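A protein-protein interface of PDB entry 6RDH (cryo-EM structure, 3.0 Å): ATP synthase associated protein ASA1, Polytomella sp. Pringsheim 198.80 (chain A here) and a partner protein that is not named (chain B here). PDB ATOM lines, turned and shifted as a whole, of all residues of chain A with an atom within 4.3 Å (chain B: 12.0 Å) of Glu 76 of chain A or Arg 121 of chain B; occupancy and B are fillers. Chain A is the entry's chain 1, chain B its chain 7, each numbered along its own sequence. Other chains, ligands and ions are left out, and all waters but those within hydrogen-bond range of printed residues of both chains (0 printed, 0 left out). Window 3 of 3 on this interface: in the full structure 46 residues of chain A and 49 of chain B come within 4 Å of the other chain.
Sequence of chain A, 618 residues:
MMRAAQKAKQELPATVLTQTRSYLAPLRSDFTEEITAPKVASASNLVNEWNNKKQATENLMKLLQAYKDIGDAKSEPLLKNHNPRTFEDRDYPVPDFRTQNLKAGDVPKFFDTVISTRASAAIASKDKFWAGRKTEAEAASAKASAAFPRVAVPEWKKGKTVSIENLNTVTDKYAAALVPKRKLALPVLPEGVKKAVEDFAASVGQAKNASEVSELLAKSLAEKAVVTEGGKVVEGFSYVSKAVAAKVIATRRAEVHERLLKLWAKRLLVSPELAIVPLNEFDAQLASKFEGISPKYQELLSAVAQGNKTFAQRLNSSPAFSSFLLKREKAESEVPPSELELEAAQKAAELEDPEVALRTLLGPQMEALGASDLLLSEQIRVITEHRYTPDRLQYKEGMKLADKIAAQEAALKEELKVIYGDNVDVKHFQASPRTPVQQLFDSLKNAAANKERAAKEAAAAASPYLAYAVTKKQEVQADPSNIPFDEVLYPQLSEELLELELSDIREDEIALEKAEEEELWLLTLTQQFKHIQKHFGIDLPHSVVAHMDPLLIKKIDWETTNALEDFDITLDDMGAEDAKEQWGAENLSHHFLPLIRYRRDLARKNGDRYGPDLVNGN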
ATOM      1  N   TYR A  67      21.633 -13.622  -6.167  1.00  0.00           N
ATOM      2  CA  TYR A  67      21.967 -13.060  -7.470  1.00  0.00           C
ATOM      3  C   TYR A  67      21.410 -11.657  -7.610  1.00  0.00           C
ATOM      4  O   TYR A  67      22.129 -10.735  -8.002  1.00  0.00           O
ATOM      5  CB  TYR A  67      21.418 -13.942  -8.584  1.00  0.00           C
ATOM      6  CG  TYR A  67      22.302 -15.095  -8.954  1.00  0.00           C
ATOM      7  CD1 TYR A  67      23.661 -14.938  -9.058  1.00  0.00           C
ATOM      8  CD2 TYR A  67      21.768 -16.338  -9.207  1.00  0.00           C
ATOM      9  CE1 TYR A  67      24.464 -15.989  -9.398  1.00  0.00           C
ATOM     10  CE2 TYR A  67      22.563 -17.389  -9.543  1.00  0.00           C
ATOM     11  CZ  TYR A  67      23.908 -17.209  -9.635  1.00  0.00           C
ATOM     12  OH  TYR A  67      24.704 -18.267  -9.967  1.00  0.00           O
ATOM     13  N   LYS A  68      20.135 -11.471  -7.265  1.00  0.00           N
ATOM     14  CA  LYS A  68      19.550 -10.137  -7.342  1.00  0.00           C
ATOM     15  C   LYS A  68      20.163  -9.180  -6.324  1.00  0.00           C
ATOM     16  O   LYS A  68      20.296  -7.982  -6.604  1.00  0.00           O
ATOM     17  CB  LYS A  68      18.044 -10.221  -7.147  1.00  0.00           C
ATOM     18  CG  LYS A  68      17.300  -9.045  -7.697  1.00  0.00           C
ATOM     19  CD  LYS A  68      15.881  -9.067  -7.234  1.00  0.00           C
ATOM     20  CE  LYS A  68      15.134  -7.858  -7.707  1.00  0.00           C
ATOM     21  NZ  LYS A  68      13.785  -7.849  -7.109  1.00  0.00           N
ATOM     22  N   GLY A  71      23.736  -8.363  -7.561  1.00  0.00           N
ATOM     23  CA  GLY A  71      23.666  -7.657  -8.816  1.00  0.00           C
ATOM     24  C   GLY A  71      23.130  -6.261  -8.623  1.00  0.00           C
ATOM     25  O   GLY A  71      23.425  -5.370  -9.416  1.00  0.00           O
ATOM     26  N   ASP A  72      22.323  -6.052  -7.591  1.00  0.00           N
ATOM     27  CA  ASP A  72      21.897  -4.705  -7.254  1.00  0.00           C
ATOM     28  C   ASP A  72      22.751  -4.078  -6.165  1.00  0.00           C
ATOM     29  O   ASP A  72      22.462  -2.959  -5.734  1.00  0.00           O
ATOM     30  CB  ASP A  72      20.431  -4.704  -6.838  1.00  0.00           C
ATOM     31  CG  ASP A  72      19.519  -5.088  -7.973  1.00  0.00           C
ATOM     32  OD1 ASP A  72      19.927  -4.920  -9.138  1.00  0.00           O
ATOM     33  OD2 ASP A  72      18.391  -5.542  -7.702  1.00  0.00           O
ATOM     34  N   LYS A  74      25.951  -3.841  -7.064  1.00  0.00           N
ATOM     35  CA  LYS A  74      26.737  -3.185  -8.091  1.00  0.00           C
ATOM     36  C   LYS A  74      25.903  -2.279  -8.980  1.00  0.00           C
ATOM     37  O   LYS A  74      26.481  -1.533  -9.777  1.00  0.00           O
ATOM     38  CB  LYS A  74      27.446  -4.240  -8.938  1.00  0.00           C
ATOM     39  CG  LYS A  74      28.094  -5.317  -8.092  1.00  0.00           C
ATOM     40  CD  LYS A  74      28.976  -6.232  -8.902  1.00  0.00           C
ATOM     41  CE  LYS A  74      29.783  -7.127  -7.988  1.00  0.00           C
ATOM     42  NZ  LYS A  74      30.525  -6.339  -6.972  1.00  0.00           N
ATOM     43  N   SER A  75      24.572  -2.338  -8.851  1.00  0.00           N
ATOM     44  CA  SER A  75      23.602  -1.500  -9.575  1.00  0.00           C
ATOM     45  C   SER A  75      23.778  -1.575 -11.087  1.00  0.00           C
ATOM     46  O   SER A  75      23.534  -0.602 -11.803  1.00  0.00           O
ATOM     47  CB  SER A  75      23.656  -0.042  -9.111  1.00  0.00           C
ATOM     48  OG  SER A  75      24.847   0.598  -9.533  1.00  0.00           O
ATOM     49  N   GLU A  76      24.199  -2.730 -11.582  1.00  0.00           N
ATOM     50  CA  GLU A  76      24.532  -2.873 -12.983  1.00  0.00           C
ATOM     51  C   GLU A  76      23.269  -2.966 -13.830  1.00  0.00           C
ATOM     52  O   GLU A  76      22.181  -3.200 -13.304  1.00  0.00           O
ATOM     53  CB  GLU A  76      25.419  -4.100 -13.171  1.00  0.00           C
ATOM     54  CG  GLU A  76      24.989  -5.320 -12.419  1.00  0.00           C
ATOM     55  CD  GLU A  76      26.110  -6.323 -12.299  1.00  0.00           C
ATOM     56  OE1 GLU A  76      27.262  -5.959 -12.604  1.00  0.00           O
ATOM     57  OE2 GLU A  76      25.845  -7.477 -11.906  1.00  0.00           O
ATOM     58  N   PRO A  77      23.377  -2.723 -15.137  1.00  0.00           N
ATOM     59  CA  PRO A  77      22.253  -2.997 -16.037  1.00  0.00           C
ATOM     60  C   PRO A  77      21.877  -4.473 -16.062  1.00  0.00           C
ATOM     61  O   PRO A  77      22.689  -5.358 -15.795  1.00  0.00           O
ATOM     62  CB  PRO A  77      22.783  -2.549 -17.401  1.00  0.00           C
ATOM     63  CG  PRO A  77      23.754  -1.506 -17.086  1.00  0.00           C
ATOM     64  CD  PRO A  77      24.412  -1.915 -15.810  1.00  0.00           C
ATOM     65  N   LEU A  78      20.613  -4.726 -16.402  1.00  0.00           N
ATOM     66  CA  LEU A  78      20.103  -6.092 -16.388  1.00  0.00           C
ATOM     67  C   LEU A  78      20.688  -6.912 -17.531  1.00  0.00           C
ATOM     68  O   LEU A  78      21.285  -7.969 -17.310  1.00  0.00           O
ATOM     69  CB  LEU A  78      18.575  -6.081 -16.459  1.00  0.00           C
ATOM     70  CG  LEU A  78      17.831  -5.793 -15.156  1.00  0.00           C
ATOM     71  CD1 LEU A  78      16.359  -5.630 -15.401  1.00  0.00           C
ATOM     72  CD2 LEU A  78      18.055  -6.903 -14.163  1.00  0.00           C
ATOM     73  N   ASN A  81      25.258  -8.164 -18.594  1.00  0.00           N
ATOM     74  CA  ASN A  81      26.071  -9.337 -18.341  1.00  0.00           C
ATOM     75  C   ASN A  81      25.603 -10.559 -19.104  1.00  0.00           C
ATOM     76  O   ASN A  81      26.333 -11.549 -19.159  1.00  0.00           O
ATOM     77  CB  ASN A  81      26.070  -9.625 -16.855  1.00  0.00           C
ATOM     78  CG  ASN A  81      26.239  -8.378 -16.041  1.00  0.00           C
ATOM     79  OD1 ASN A  81      25.331  -7.963 -15.327  1.00  0.00           O
ATOM     80  ND2 ASN A  81      27.404  -7.757 -16.149  1.00  0.00           N
ATOM     81  N   TRP A 130      30.297 -15.364 -15.402  1.00  0.00           N
ATOM     82  CA  TRP A 130      29.153 -15.974 -14.740  1.00  0.00           C
ATOM     83  C   TRP A 130      29.575 -17.052 -13.761  1.00  0.00           C
ATOM     84  O   TRP A 130      28.893 -17.257 -12.757  1.00  0.00           O
ATOM     85  CB  TRP A 130      28.160 -16.527 -15.753  1.00  0.00           C
ATOM     86  CG  TRP A 130      27.176 -15.499 -16.206  1.00  0.00           C
ATOM     87  CD1 TRP A 130      26.990 -15.078 -17.474  1.00  0.00           C
ATOM     88  CD2 TRP A 130      26.259 -14.746 -15.394  1.00  0.00           C
ATOM     89  NE1 TRP A 130      26.016 -14.120 -17.517  1.00  0.00           N
ATOM     90  CE2 TRP A 130      25.552 -13.901 -16.251  1.00  0.00           C
ATOM     91  CE3 TRP A 130      25.961 -14.715 -14.031  1.00  0.00           C
ATOM     92  CZ2 TRP A 130      24.578 -13.035 -15.799  1.00  0.00           C
ATOM     93  CZ3 TRP A 130      25.000 -13.853 -13.588  1.00  0.00           C
ATOM     94  CH2 TRP A 130      24.319 -13.024 -14.464  1.00  0.00           C
ATOM     95  N   ARG A 133      30.484 -14.975 -10.743  1.00  0.00           N
ATOM     96  CA  ARG A 133      29.267 -14.496 -10.096  1.00  0.00           C
ATOM     97  C   ARG A 133      28.552 -15.621  -9.364  1.00  0.00           C
ATOM     98  O   ARG A 133      28.021 -15.414  -8.266  1.00  0.00           O
ATOM     99  CB  ARG A 133      28.348 -13.863 -11.135  1.00  0.00           C
ATOM    100  CG  ARG A 133      26.983 -13.512 -10.626  1.00  0.00           C
ATOM    101  CD  ARG A 133      27.067 -12.353  -9.707  1.00  0.00           C
ATOM    102  NE  ARG A 133      26.943 -11.108 -10.438  1.00  0.00           N
ATOM    103  CZ  ARG A 133      27.617 -10.014 -10.135  1.00  0.00           C
ATOM    104  NH1 ARG A 133      28.471 -10.032  -9.125  1.00  0.00           N
ATOM    105  NH2 ARG A 133      27.453  -8.914 -10.851  1.00  0.00           N
ATOM    106  N   THR B 112       6.772 -16.210  -6.829  1.00  0.00           N
ATOM    107  CA  THR B 112       7.243 -14.904  -6.394  1.00  0.00           C
ATOM    108  C   THR B 112       8.654 -14.583  -6.878  1.00  0.00           C
ATOM    109  O   THR B 112       9.242 -13.609  -6.405  1.00  0.00           O
ATOM    110  CB  THR B 112       7.195 -14.812  -4.871  1.00  0.00           C
ATOM    111  OG1 THR B 112       8.209 -15.651  -4.312  1.00  0.00           O
ATOM    112  CG2 THR B 112       5.856 -15.264  -4.364  1.00  0.00           C
ATOM    113  N   MET B 113       9.217 -15.380  -7.786  1.00  0.00           N
ATOM    114  CA  MET B 113      10.535 -15.138  -8.352  1.00  0.00           C
ATOM    115  C   MET B 113      10.540 -15.379  -9.853  1.00  0.00           C
ATOM    116  O   MET B 113      11.561 -15.778 -10.415  1.00  0.00           O
ATOM    117  CB  MET B 113      11.590 -16.012  -7.685  1.00  0.00           C
ATOM    118  CG  MET B 113      11.939 -15.566  -6.301  1.00  0.00           C
ATOM    119  SD  MET B 113      13.381 -16.361  -5.621  1.00  0.00           S
ATOM    120  CE  MET B 113      13.538 -15.423  -4.110  1.00  0.00           C
ATOM    121  N   TYR B 114       9.413 -15.149 -10.514  1.00  0.00           N
ATOM    122  CA  TYR B 114       9.319 -15.318 -11.954  1.00  0.00           C
ATOM    123  C   TYR B 114       9.636 -14.051 -12.725  1.00  0.00           C
ATOM    124  O   TYR B 114       9.859 -14.130 -13.937  1.00  0.00           O
ATOM    125  CB  TYR B 114       7.917 -15.778 -12.354  1.00  0.00           C
ATOM    126  CG  TYR B 114       7.684 -17.255 -12.266  1.00  0.00           C
ATOM    127  CD1 TYR B 114       8.705 -18.126 -11.948  1.00  0.00           C
ATOM    128  CD2 TYR B 114       6.442 -17.780 -12.547  1.00  0.00           C
ATOM    129  CE1 TYR B 114       8.484 -19.473 -11.884  1.00  0.00           C
ATOM    130  CE2 TYR B 114       6.213 -19.123 -12.490  1.00  0.00           C
ATOM    131  CZ  TYR B 114       7.237 -19.963 -12.162  1.00  0.00           C
ATOM    132  OH  TYR B 114       6.999 -21.308 -12.104  1.00  0.00           O
ATOM    133  N   GLY B 115       9.652 -12.901 -12.058  1.00  0.00           N
ATOM    134  CA  GLY B 115       9.777 -11.641 -12.752  1.00  0.00           C
ATOM    135  C   GLY B 115      11.139 -11.443 -13.380  1.00  0.00           C
ATOM    136  O   GLY B 115      12.128 -12.065 -13.005  1.00  0.00           O
ATOM    137  N   LYS B 116      11.182 -10.540 -14.358  1.00  0.00           N
ATOM    138  CA  LYS B 116      12.373 -10.385 -15.179  1.00  0.00           C
ATOM    139  C   LYS B 116      13.524  -9.725 -14.446  1.00  0.00           C
ATOM    140  O   LYS B 116      14.648  -9.768 -14.947  1.00  0.00           O
ATOM    141  CB  LYS B 116      12.046  -9.598 -16.440  1.00  0.00           C
ATOM    142  CG  LYS B 116      11.194 -10.371 -17.407  1.00  0.00           C
ATOM    143  CD  LYS B 116      10.784  -9.520 -18.574  1.00  0.00           C
ATOM    144  CE  LYS B 116       9.967 -10.327 -19.558  1.00  0.00           C
ATOM    145  NZ  LYS B 116       9.540  -9.495 -20.710  1.00  0.00           N
ATOM    146  N   ASP B 117      13.290  -9.128 -13.281  1.00  0.00           N
ATOM    147  CA  ASP B 117      14.413  -8.709 -12.463  1.00  0.00           C
ATOM    148  C   ASP B 117      15.099  -9.892 -11.809  1.00  0.00           C
ATOM    149  O   ASP B 117      16.257  -9.772 -11.412  1.00  0.00           O
ATOM    150  CB  ASP B 117      13.969  -7.712 -11.400  1.00  0.00           C
ATOM    151  CG  ASP B 117      12.688  -8.114 -10.729  1.00  0.00           C
ATOM    152  OD1 ASP B 117      12.117  -9.149 -11.114  1.00  0.00           O
ATOM    153  OD2 ASP B 117      12.242  -7.392  -9.818  1.00  0.00           O
ATOM    154  N   PHE B 118      14.413 -11.025 -11.677  1.00  0.00           N
ATOM    155  CA  PHE B 118      15.058 -12.256 -11.250  1.00  0.00           C
ATOM    156  C   PHE B 118      15.572 -13.071 -12.419  1.00  0.00           C
ATOM    157  O   PHE B 118      16.424 -13.941 -12.220  1.00  0.00           O
ATOM    158  CB  PHE B 118      14.092 -13.119 -10.447  1.00  0.00           C
ATOM    159  CG  PHE B 118      13.844 -12.624  -9.066  1.00  0.00           C
ATOM    160  CD1 PHE B 118      14.715 -12.935  -8.046  1.00  0.00           C
ATOM    161  CD2 PHE B 118      12.730 -11.864  -8.787  1.00  0.00           C
ATOM    162  CE1 PHE B 118      14.486 -12.489  -6.778  1.00  0.00           C
ATOM    163  CE2 PHE B 118      12.492 -11.414  -7.519  1.00  0.00           C
ATOM    164  CZ  PHE B 118      13.371 -11.728  -6.511  1.00  0.00           C
ATOM    165  N   TYR B 119      15.062 -12.816 -13.621  1.00  0.00           N
ATOM    166  CA  TYR B 119      15.514 -13.530 -14.806  1.00  0.00           C
ATOM    167  C   TYR B 119      16.934 -13.138 -15.161  1.00  0.00           C
ATOM    168  O   TYR B 119      17.788 -13.998 -15.391  1.00  0.00           O
ATOM    169  CB  TYR B 119      14.571 -13.224 -15.969  1.00  0.00           C
ATOM    170  CG  TYR B 119      14.683 -14.100 -17.191  1.00  0.00           C
ATOM    171  CD1 TYR B 119      15.712 -13.934 -18.100  1.00  0.00           C
ATOM    172  CD2 TYR B 119      13.725 -15.046 -17.467  1.00  0.00           C
ATOM    173  CE1 TYR B 119      15.813 -14.711 -19.204  1.00  0.00           C
ATOM    174  CE2 TYR B 119      13.820 -15.832 -18.580  1.00  0.00           C
ATOM    175  CZ  TYR B 119      14.864 -15.651 -19.441  1.00  0.00           C
ATOM    176  OH  TYR B 119      14.979 -16.415 -20.561  1.00  0.00           O
ATOM    177  N   TYR B 120      17.199 -11.842 -15.234  1.00  0.00           N
ATOM    178  CA  TYR B 120      18.444 -11.358 -15.797  1.00  0.00           C
ATOM    179  C   TYR B 120      19.545 -11.204 -14.769  1.00  0.00           C
ATOM    180  O   TYR B 120      20.711 -11.103 -15.151  1.00  0.00           O
ATOM    181  CB  TYR B 120      18.205 -10.032 -16.515  1.00  0.00           C
ATOM    182  CG  TYR B 120      17.347 -10.196 -17.735  1.00  0.00           C
ATOM    183  CD1 TYR B 120      17.770 -10.974 -18.796  1.00  0.00           C
ATOM    184  CD2 TYR B 120      16.117  -9.581 -17.826  1.00  0.00           C
ATOM    185  CE1 TYR B 120      16.987 -11.140 -19.904  1.00  0.00           C
ATOM    186  CE2 TYR B 120      15.329  -9.740 -18.936  1.00  0.00           C
ATOM    187  CZ  TYR B 120      15.769 -10.513 -19.968  1.00  0.00           C
ATOM    188  OH  TYR B 120      14.979 -10.670 -21.074  1.00  0.00           O
ATOM    189  N   ARG B 121      19.223 -11.192 -13.484  1.00  0.00           N
ATOM    190  CA  ARG B 121      20.287 -11.203 -12.498  1.00  0.00           C
ATOM    191  C   ARG B 121      20.901 -12.579 -12.334  1.00  0.00           C
ATOM    192  O   ARG B 121      22.042 -12.685 -11.881  1.00  0.00           O
ATOM    193  CB  ARG B 121      19.771 -10.722 -11.150  1.00  0.00           C
ATOM    194  CG  ARG B 121      19.415  -9.269 -11.109  1.00  0.00           C
ATOM    195  CD  ARG B 121      20.568  -8.390 -11.470  1.00  0.00           C
ATOM    196  NE  ARG B 121      20.193  -6.990 -11.346  1.00  0.00           N
ATOM    197  CZ  ARG B 121      20.771  -6.012 -12.025  1.00  0.00           C
ATOM    198  NH1 ARG B 121      21.739  -6.293 -12.880  1.00  0.00           N
ATOM    199  NH2 ARG B 121      20.372  -4.762 -11.860  1.00  0.00           N
ATOM    200  N   ALA B 122      20.186 -13.624 -12.713  1.00  0.00           N
ATOM    201  CA  ALA B 122      20.592 -14.980 -12.401  1.00  0.00           C
ATOM    202  C   ALA B 122      21.431 -15.585 -13.509  1.00  0.00           C
ATOM    203  O   ALA B 122      21.261 -15.270 -14.687  1.00  0.00           O
ATOM    204  CB  ALA B 122      19.370 -15.857 -12.155  1.00  0.00           C
ATOM    205  N   HIS B 123      22.346 -16.454 -13.100  1.00  0.00           N
ATOM    206  CA  HIS B 123      23.089 -17.316 -14.002  1.00  0.00           C
ATOM    207  C   HIS B 123      22.111 -18.136 -14.835  1.00  0.00           C
ATOM    208  O   HIS B 123      21.063 -18.537 -14.324  1.00  0.00           O
ATOM    209  CB  HIS B 123      23.980 -18.233 -13.167  1.00  0.00           C
ATOM    210  CG  HIS B 123      24.959 -19.046 -13.947  1.00  0.00           C
ATOM    211  ND1 HIS B 123      26.313 -18.820 -13.892  1.00  0.00           N
ATOM    212  CD2 HIS B 123      24.791 -20.125 -14.745  1.00  0.00           C
ATOM    213  CE1 HIS B 123      26.937 -19.703 -14.648  1.00  0.00           C
ATOM    214  NE2 HIS B 123      26.035 -20.505 -15.180  1.00  0.00           N
ATOM    215  N   PRO B 124      22.396 -18.365 -16.120  1.00  0.00           N
ATOM    216  CA  PRO B 124      21.423 -19.069 -16.973  1.00  0.00           C
ATOM    217  C   PRO B 124      21.140 -20.501 -16.561  1.00  0.00           C
ATOM    218  O   PRO B 124      19.982 -20.930 -16.606  1.00  0.00           O
ATOM    219  CB  PRO B 124      22.079 -19.003 -18.354  1.00  0.00           C
ATOM    220  CG  PRO B 124      22.919 -17.797 -18.293  1.00  0.00           C
ATOM    221  CD  PRO B 124      23.453 -17.725 -16.915  1.00  0.00           C
ATOM    222  N   GLU B 125      22.157 -21.246 -16.139  1.00  0.00           N
ATOM    223  CA  GLU B 125      21.931 -22.625 -15.733  1.00  0.00           C
ATOM    224  C   GLU B 125      21.184 -22.710 -14.413  1.00  0.00           C
ATOM    225  O   GLU B 125      20.397 -23.640 -14.212  1.00  0.00           O
ATOM    226  CB  GLU B 125      23.257 -23.367 -15.654  1.00  0.00           C
ATOM    227  CG  GLU B 125      24.039 -23.302 -16.949  1.00  0.00           C
ATOM    228  CD  GLU B 125      23.254 -23.838 -18.137  1.00  0.00           C
ATOM    229  OE1 GLU B 125      22.685 -24.942 -18.032  1.00  0.00           O
ATOM    230  OE2 GLU B 125      23.205 -23.152 -19.179  1.00  0.00           O
ATOM    231  N   ASP B 126      21.373 -21.735 -13.526  1.00  0.00           N
ATOM    232  CA  ASP B 126      20.598 -21.721 -12.294  1.00  0.00           C
ATOM    233  C   ASP B 126      19.147 -21.356 -12.551  1.00  0.00           C
ATOM    234  O   ASP B 126      18.256 -21.895 -11.893  1.00  0.00           O
ATOM    235  CB  ASP B 126      21.222 -20.767 -11.288  1.00  0.00           C
ATOM    236  CG  ASP B 126      22.536 -21.275 -10.763  1.00  0.00           C
ATOM    237  OD1 ASP B 126      22.773 -22.493 -10.859  1.00  0.00           O
ATOM    238  OD2 ASP B 126      23.332 -20.466 -10.252  1.00  0.00           O
ATOM    239  N   LEU B 127      18.880 -20.483 -13.515  1.00  0.00           N
ATOM    240  CA  LEU B 127      17.494 -20.205 -13.862  1.00  0.00           C
ATOM    241  C   LEU B 127      16.839 -21.387 -14.566  1.00  0.00           C
ATOM    242  O   LEU B 127      15.643 -21.631 -14.377  1.00  0.00           O
ATOM    243  CB  LEU B 127      17.409 -18.972 -14.748  1.00  0.00           C
ATOM    244  CG  LEU B 127      16.005 -18.406 -14.810  1.00  0.00           C
ATOM    245  CD1 LEU B 127      15.745 -17.607 -13.563  1.00  0.00           C
ATOM    246  CD2 LEU B 127      15.810 -17.592 -16.037  1.00  0.00           C
ATOM    247  N   LYS B 128      17.601 -22.140 -15.356  1.00  0.00           N
ATOM    248  CA  LYS B 128      17.053 -23.350 -15.956  1.00  0.00           C
ATOM    249  C   LYS B 128      16.758 -24.407 -14.900  1.00  0.00           C
ATOM    250  O   LYS B 128      15.735 -25.097 -14.973  1.00  0.00           O
ATOM    251  CB  LYS B 128      18.014 -23.888 -17.005  1.00  0.00           C
ATOM    252  CG  LYS B 128      18.044 -23.041 -18.255  1.00  0.00           C
ATOM    253  CD  LYS B 128      18.813 -23.697 -19.372  1.00  0.00           C
ATOM    254  CE  LYS B 128      18.689 -22.875 -20.632  1.00  0.00           C
ATOM    255  NZ  LYS B 128      19.194 -21.502 -20.404  1.00  0.00           N
ATOM    256  N   PHE B 130      15.953 -23.651 -11.833  1.00  0.00           N
ATOM    257  CA  PHE B 130      14.813 -23.134 -11.087  1.00  0.00           C
ATOM    258  C   PHE B 130      13.506 -23.401 -11.816  1.00  0.00           C
ATOM    259  O   PHE B 130      12.508 -23.787 -11.194  1.00  0.00           O
ATOM    260  CB  PHE B 130      15.019 -21.646 -10.845  1.00  0.00           C
ATOM    261  CG  PHE B 130      13.865 -20.965 -10.204  1.00  0.00           C
ATOM    262  CD1 PHE B 130      13.598 -21.146  -8.868  1.00  0.00           C
ATOM    263  CD2 PHE B 130      13.070 -20.108 -10.932  1.00  0.00           C
ATOM    264  CE1 PHE B 130      12.548 -20.504  -8.280  1.00  0.00           C
ATOM    265  CE2 PHE B 130      12.016 -19.468 -10.349  1.00  0.00           C
ATOM    266  CZ  PHE B 130      11.759 -19.660  -9.023  1.00  0.00           C
ATOM    267  N   TYR B 131      13.497 -23.234 -13.136  1.00  0.00           N
ATOM    268  CA  TYR B 131      12.282 -23.518 -13.890  1.00  0.00           C
ATOM    269  C   TYR B 131      12.004 -25.016 -13.953  1.00  0.00           C
ATOM    270  O   TYR B 131      10.836 -25.433 -13.947  1.00  0.00           O
ATOM    271  CB  TYR B 131      12.381 -22.924 -15.291  1.00  0.00           C
ATOM    272  CG  TYR B 131      12.145 -21.432 -15.362  1.00  0.00           C
ATOM    273  CD1 TYR B 131      12.181 -20.763 -16.573  1.00  0.00           C
ATOM    274  CD2 TYR B 131      11.881 -20.694 -14.222  1.00  0.00           C
ATOM    275  CE1 TYR B 131      11.961 -19.406 -16.638  1.00  0.00           C
ATOM    276  CE2 TYR B 131      11.670 -19.347 -14.281  1.00  0.00           C
ATOM    277  CZ  TYR B 131      11.708 -18.709 -15.484  1.00  0.00           C
ATOM    278  OH  TYR B 131      11.486 -17.360 -15.515  1.00  0.00           O
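The side-chain hydroxyl of Tyr 67 of chain A lies within hydrogen-bond range of the side-chain carboxylate of Asp 126 of chain B (2.6 Å). The side-chain carboxylate (OD2) of Asp 117 of chain B lies within salt-bridge range of the side-chain amino group (NZ) of Lys 68 of chain A (3.2 Å). The guanidinium group (NH2) of Arg 121 of chain B is in salt-bridge range of the side-chain carboxylate (OD1) of Asp 72 of chain A (2.8 Å). The backbone carbonyl oxygen (O) of Glu 76 of chain A sits at hydrogen-bond distance from the guanidinium group (NH2) of Arg 121 of chain B (2.8 Å). The guanidinium group (NH1) of Arg 121 of chain B is in hydrogen-bond range of the backbone carbonyl oxygen (O) of Pro 77 of chain A. ND1 of His 123 of chain B sits at hydrogen-bond distance from O of Trp 130 of chain A, 3.2 Å away.
Of chain B, only Arg 121 (3.6 Å), Ala 122 (3.7 Å), His 123 (3.3 Å) and Asp 126 (2.6 Å) come within 4 Å of Tyr 67 of chain A. Asp 72 of chain A touches one residue of chain B. Lys 74 of chain A touches none of the printed residues of chain B. Pro 77 of chain A touches just one residue of chain B: Arg 121. Leu 78 of chain A touches just these residues of chain B: Tyr 120 (3.8 Å) and Arg 121 (3.5 Å). Met 113 of chain B touches none of the printed residues of chain A. Tyr 114 of chain B touches none of the printed residues of chain A. Printed residues of chain A within 4 Å of Asp 117 of chain B: Lys 68. Of chain A, only Tyr 67, Lys 68, Gly 71, Asp 72, Glu 76, Pro 77, Leu 78 and Trp 130 come within 4 Å of Arg 121 of chain B. Of the printed residues of chain A, Asp 126 of chain B touches Tyr 67. The nearest residue of chain B that does not touch Glu 76 of chain A is Tyr 120 of chain B (7.1 Å). The nearest printed residue of chain A that does not touch Arg 121 of chain B is Asn 81 of chain A (4.7 Å).
The side-chain amide oxygen (OD1) of Asn 81 of chain A lies close to the side-chain carboxylate (OE2) of Glu 76 of chain A. The guanidinium group (NH2) of Arg 133 of chain A is in salt-bridge range of the side-chain carboxylate (OE2) of Glu 76 of chain A (2.4 Å). The backbone carbonyl oxygen of Asn 81 of chain A lies within hydrogen-bond range of the indole nitrogen of Trp 130 of chain A (3.1 Å).
Of the 19 printed residues of chain B, 7 touch a printed residue of chain A. Hydrophobic or aromatic side chains of chain B within 4 Å of the printed part of chain A: Phe 118, Tyr 120, Ala 122 and His 123. Of the 12 printed residues of chain A, 8 touch a printed residue of chain B. Printed residues of chain A that touch a printed residue of chain B: Tyr 67, Lys 68, Gly 71, Asp 72, Glu 76, Pro 77, Leu 78 and Trp 130. Along chain A the printed residues that touch a printed residue of chain B span positions 67 to 130.
Arg 121 of chain B touches Tyr 67 of chain A (O to CB, 3.6 Å). Tyr 67 of chain A touches Ala 122 of chain B. CB of His 123 of chain B touches OH of Tyr 67 of chain A (3.3 Å). Lys 68 of chain A touches Phe 118 of chain B (CD to CE1, 3.7 Å). CA of Lys 68 of chain A touches CB of Arg 121 of chain B, 3.9 Å away. CZ of Arg 121 of chain B touches O of Gly 71 of chain A, 3.8 Å away. Tyr 120 of chain B touches Leu 78 of chain A. CD2 of Leu 78 of chain A touches NE of Arg 121 of chain B (3.5 Å). Trp 130 of chain A touches Arg 121 of chain B (CH2 to O, 3.5 Å). Trp 130 of chain A touches Ala 122 of chain B.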
